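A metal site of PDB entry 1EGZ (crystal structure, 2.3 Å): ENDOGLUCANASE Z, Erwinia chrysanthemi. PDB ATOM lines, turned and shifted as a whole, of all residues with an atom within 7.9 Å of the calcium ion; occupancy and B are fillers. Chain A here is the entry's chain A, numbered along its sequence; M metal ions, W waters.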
ATOM      1  N   ALA A 117      -6.243 -15.224 -18.428  1.00  0.00           N
ATOM      2  CA  ALA A 117      -7.107 -15.405 -19.590  1.00  0.00           C
ATOM      3  C   ALA A 117      -7.698 -14.080 -20.025  1.00  0.00           C
ATOM      4  O   ALA A 117      -7.747 -13.755 -21.208  1.00  0.00           O
ATOM      5  CB  ALA A 117      -8.217 -16.400 -19.287  1.00  0.00           C
ATOM      6  N   TYR A 120      -4.520 -11.928 -21.367  1.00  0.00           N
ATOM      7  CA  TYR A 120      -3.863 -12.370 -22.600  1.00  0.00           C
ATOM      8  C   TYR A 120      -4.684 -13.184 -23.572  1.00  0.00           C
ATOM      9  O   TYR A 120      -4.234 -13.485 -24.662  1.00  0.00           O
ATOM     10  CB  TYR A 120      -2.607 -13.152 -22.253  1.00  0.00           C
ATOM     11  CG  TYR A 120      -1.588 -12.320 -21.510  1.00  0.00           C
ATOM     12  CD1 TYR A 120      -0.895 -11.303 -22.167  1.00  0.00           C
ATOM     13  CD2 TYR A 120      -1.320 -12.539 -20.165  1.00  0.00           C
ATOM     14  CE1 TYR A 120       0.040 -10.514 -21.493  1.00  0.00           C
ATOM     15  CE2 TYR A 120      -0.389 -11.762 -19.482  1.00  0.00           C
ATOM     16  CZ  TYR A 120       0.288 -10.758 -20.152  1.00  0.00           C
ATOM     17  OH  TYR A 120       1.210  -9.974 -19.489  1.00  0.00           O
ATOM     18  N   GLY A 121      -5.917 -13.486 -23.186  1.00  0.00           N
ATOM     19  CA  GLY A 121      -6.789 -14.282 -24.024  1.00  0.00           C
ATOM     20  C   GLY A 121      -6.839 -14.001 -25.518  1.00  0.00           C
ATOM     21  O   GLY A 121      -7.083 -14.927 -26.282  1.00  0.00           O
ATOM     22  N   ASN A 122      -6.624 -12.774 -25.963  1.00  0.00           N
ATOM     23  CA  ASN A 122      -6.699 -12.485 -27.385  1.00  0.00           C
ATOM     24  C   ASN A 122      -5.430 -12.517 -28.181  1.00  0.00           C
ATOM     25  O   ASN A 122      -5.470 -12.393 -29.408  1.00  0.00           O
ATOM     26  CB  ASN A 122      -7.440 -11.186 -27.653  1.00  0.00           C
ATOM     27  CG  ASN A 122      -8.909 -11.403 -27.883  1.00  0.00           C
ATOM     28  OD1 ASN A 122      -9.302 -11.910 -28.943  1.00  0.00           O
ATOM     29  ND2 ASN A 122      -9.726 -11.099 -26.887  1.00  0.00           N
ATOM     30  N   LYS A 123      -4.294 -12.656 -27.526  1.00  0.00           N
ATOM     31  CA  LYS A 123      -3.054 -12.717 -28.277  1.00  0.00           C
ATOM     32  C   LYS A 123      -2.802 -14.182 -28.628  1.00  0.00           C
ATOM     33  O   LYS A 123      -2.969 -15.071 -27.793  1.00  0.00           O
ATOM     34  CB  LYS A 123      -1.901 -12.106 -27.487  1.00  0.00           C
ATOM     35  CG  LYS A 123      -1.732 -10.602 -27.734  1.00  0.00           C
ATOM     36  CD  LYS A 123      -2.913  -9.798 -27.226  1.00  0.00           C
ATOM     37  CE  LYS A 123      -2.999  -8.427 -27.912  1.00  0.00           C
ATOM     38  NZ  LYS A 123      -3.404  -8.505 -29.368  1.00  0.00           N
ATOM     39  N   PRO A 124      -2.468 -14.454 -29.887  1.00  0.00           N
ATOM     40  CA  PRO A 124      -2.219 -15.830 -30.304  1.00  0.00           C
ATOM     41  C   PRO A 124      -0.935 -16.454 -29.738  1.00  0.00           C
ATOM     42  O   PRO A 124      -0.667 -17.632 -29.961  1.00  0.00           O
ATOM     43  CB  PRO A 124      -2.170 -15.710 -31.835  1.00  0.00           C
ATOM     44  CG  PRO A 124      -1.608 -14.329 -32.048  1.00  0.00           C
ATOM     45  CD  PRO A 124      -2.388 -13.523 -31.030  1.00  0.00           C
ATOM     46  N   VAL A 126      -0.043 -16.693 -26.335  1.00  0.00           N
ATOM     47  CA  VAL A 126      -0.208 -17.355 -25.047  1.00  0.00           C
ATOM     48  C   VAL A 126      -0.750 -18.795 -25.046  1.00  0.00           C
ATOM     49  O   VAL A 126      -1.691 -19.128 -25.777  1.00  0.00           O
ATOM     50  CB  VAL A 126      -1.051 -16.449 -24.103  1.00  0.00           C
ATOM     51  CG1 VAL A 126      -1.206 -17.065 -22.726  1.00  0.00           C
ATOM     52  CG2 VAL A 126      -0.373 -15.089 -23.995  1.00  0.00           C
ATOM     53  N   TYR A 128      -1.574 -22.009 -22.035  1.00  0.00           N
ATOM     54  CA  TYR A 128      -1.716 -22.254 -20.587  1.00  0.00           C
ATOM     55  C   TYR A 128      -1.264 -23.656 -20.217  1.00  0.00           C
ATOM     56  O   TYR A 128      -1.633 -24.619 -20.865  1.00  0.00           O
ATOM     57  CB  TYR A 128      -3.177 -22.111 -20.149  1.00  0.00           C
ATOM     58  CG  TYR A 128      -3.846 -20.875 -20.650  1.00  0.00           C
ATOM     59  CD1 TYR A 128      -3.581 -19.634 -20.068  1.00  0.00           C
ATOM     60  CD2 TYR A 128      -4.732 -20.923 -21.719  1.00  0.00           C
ATOM     61  CE1 TYR A 128      -4.172 -18.474 -20.550  1.00  0.00           C
ATOM     62  CE2 TYR A 128      -5.332 -19.759 -22.211  1.00  0.00           C
ATOM     63  CZ  TYR A 128      -5.042 -18.539 -21.622  1.00  0.00           C
ATOM     64  OH  TYR A 128      -5.636 -17.390 -22.095  1.00  0.00           O
ATOM     65  N   ARG A 155     -11.944 -21.498 -20.685  1.00  0.00           N
ATOM     66  CA  ARG A 155     -12.793 -21.487 -21.866  1.00  0.00           C
ATOM     67  C   ARG A 155     -13.953 -20.499 -21.854  1.00  0.00           C
ATOM     68  O   ARG A 155     -14.420 -20.079 -22.913  1.00  0.00           O
ATOM     69  CB  ARG A 155     -13.289 -22.902 -22.185  1.00  0.00           C
ATOM     70  CG  ARG A 155     -12.207 -23.820 -22.763  1.00  0.00           C
ATOM     71  CD  ARG A 155     -11.709 -23.344 -24.140  1.00  0.00           C
ATOM     72  NE  ARG A 155     -10.608 -24.161 -24.652  1.00  0.00           N
ATOM     73  CZ  ARG A 155      -9.425 -23.679 -25.029  1.00  0.00           C
ATOM     74  NH1 ARG A 155      -9.176 -22.377 -24.964  1.00  0.00           N
ATOM     75  NH2 ARG A 155      -8.479 -24.494 -25.460  1.00  0.00           N
ATOM     76  N   ILE A 157     -13.735 -17.523 -20.732  1.00  0.00           N
ATOM     77  CA  ILE A 157     -13.100 -16.250 -21.044  1.00  0.00           C
ATOM     78  C   ILE A 157     -12.371 -16.310 -22.386  1.00  0.00           C
ATOM     79  O   ILE A 157     -12.602 -15.479 -23.274  1.00  0.00           O
ATOM     80  CB  ILE A 157     -12.069 -15.873 -19.940  1.00  0.00           C
ATOM     81  CG1 ILE A 157     -12.756 -15.789 -18.573  1.00  0.00           C
ATOM     82  CG2 ILE A 157     -11.389 -14.562 -20.255  1.00  0.00           C
ATOM     83  CD1 ILE A 157     -11.797 -15.728 -17.420  1.00  0.00           C
ATOM     84  N   ASP A 158     -11.482 -17.295 -22.521  1.00  0.00           N
ATOM     85  CA  ASP A 158     -10.654 -17.540 -23.701  1.00  0.00           C
ATOM     86  C   ASP A 158     -11.053 -18.919 -24.256  1.00  0.00           C
ATOM     87  O   ASP A 158     -10.556 -19.949 -23.814  1.00  0.00           O
ATOM     88  CB  ASP A 158      -9.192 -17.516 -23.269  1.00  0.00           C
ATOM     89  CG  ASP A 158      -8.217 -17.656 -24.430  1.00  0.00           C
ATOM     90  OD1 ASP A 158      -8.589 -17.513 -25.606  1.00  0.00           O
ATOM     91  OD2 ASP A 158      -7.032 -17.873 -24.132  1.00  0.00           O
ATOM     92  N   PRO A 159     -11.890 -18.923 -25.307  1.00  0.00           N
ATOM     93  CA  PRO A 159     -12.415 -20.103 -25.993  1.00  0.00           C
ATOM     94  C   PRO A 159     -11.501 -20.875 -26.934  1.00  0.00           C
ATOM     95  O   PRO A 159     -11.856 -21.979 -27.352  1.00  0.00           O
ATOM     96  CB  PRO A 159     -13.559 -19.503 -26.795  1.00  0.00           C
ATOM     97  CG  PRO A 159     -12.937 -18.241 -27.270  1.00  0.00           C
ATOM     98  CD  PRO A 159     -12.338 -17.698 -25.990  1.00  0.00           C
ATOM     99  N   ASP A 160     -10.339 -20.339 -27.262  1.00  0.00           N
ATOM    100  CA  ASP A 160      -9.504 -21.033 -28.231  1.00  0.00           C
ATOM    101  C   ASP A 160      -8.015 -21.227 -27.978  1.00  0.00           C
ATOM    102  O   ASP A 160      -7.381 -21.946 -28.730  1.00  0.00           O
ATOM    103  CB  ASP A 160      -9.667 -20.353 -29.590  1.00  0.00           C
ATOM    104  CG  ASP A 160      -9.235 -18.896 -29.569  1.00  0.00           C
ATOM    105  OD1 ASP A 160      -9.754 -18.140 -28.718  1.00  0.00           O
ATOM    106  OD2 ASP A 160      -8.378 -18.509 -30.390  1.00  0.00           O
ATOM    107  N   ASN A 161      -7.449 -20.559 -26.981  1.00  0.00           N
ATOM    108  CA  ASN A 161      -6.008 -20.707 -26.761  1.00  0.00           C
ATOM    109  C   ASN A 161      -5.675 -22.061 -26.151  1.00  0.00           C
ATOM    110  O   ASN A 161      -6.379 -22.560 -25.276  1.00  0.00           O
ATOM    111  CB  ASN A 161      -5.425 -19.565 -25.919  1.00  0.00           C
ATOM    112  CG  ASN A 161      -5.254 -18.294 -26.722  1.00  0.00           C
ATOM    113  OD1 ASN A 161      -6.240 -17.665 -27.153  1.00  0.00           O
ATOM    114  ND2 ASN A 161      -4.018 -17.891 -26.939  1.00  0.00           N
ATOM    115  N   LEU A 162      -4.598 -22.654 -26.656  1.00  0.00           N
ATOM    116  CA  LEU A 162      -4.098 -23.961 -26.250  1.00  0.00           C
ATOM    117  C   LEU A 162      -3.917 -24.122 -24.734  1.00  0.00           C
ATOM    118  O   LEU A 162      -3.346 -23.247 -24.078  1.00  0.00           O
ATOM    119  CB  LEU A 162      -2.772 -24.254 -26.977  1.00  0.00           C
ATOM    120  CG  LEU A 162      -2.148 -25.646 -26.857  1.00  0.00           C
ATOM    121  CD1 LEU A 162      -3.111 -26.672 -27.409  1.00  0.00           C
ATOM    122  CD2 LEU A 162      -0.823 -25.706 -27.617  1.00  0.00           C
HETATM  123 CA    CA M   1      -8.086 -16.475 -27.376  1.00  0.00          CA
HETATM  124  O   HOH W   1      -7.076 -15.260 -29.661  1.00  0.00           O
HETATM  125  O   HOH W   2      -9.930 -15.395 -27.202  1.00  0.00           O
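OD1 of Asp 158 is bound to the calcium ion.
Water W2 is bound to the calcium ion, 2.1 Å away.
O of Gly 121 binds the calcium ion, at 2.1 Å.
The calcium ion is bound by OD1 of Asn 161 (2.2 Å).
OD1 of Asp 160 is bound to the calcium ion.
The calcium ion is bound by water W1 (2.8 Å).
Of the 15 residues printed, 4 come within 4 Å of the calcium ion.
OD2 of Asp 158 is in hydrogen-bond range of OH of Tyr 128 (2.5 Å).
The backbone carbonyl oxygen (O) of Asp 158 is in hydrogen-bond range of the guanidinium group (NH1) of Arg 155, 3.0 Å away.
The side-chain amide nitrogen (ND2) of Asn 161 sits at hydrogen-bond distance from the backbone carbonyl oxygen (O) of Lys 123 (3.1 Å).
O of Asn 161 lies within hydrogen-bond range of NH1 of Arg 155 (2.8 Å).
O of Val 126 is in hydrogen-bond range of ND2 of Asn 161 (2.9 Å).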
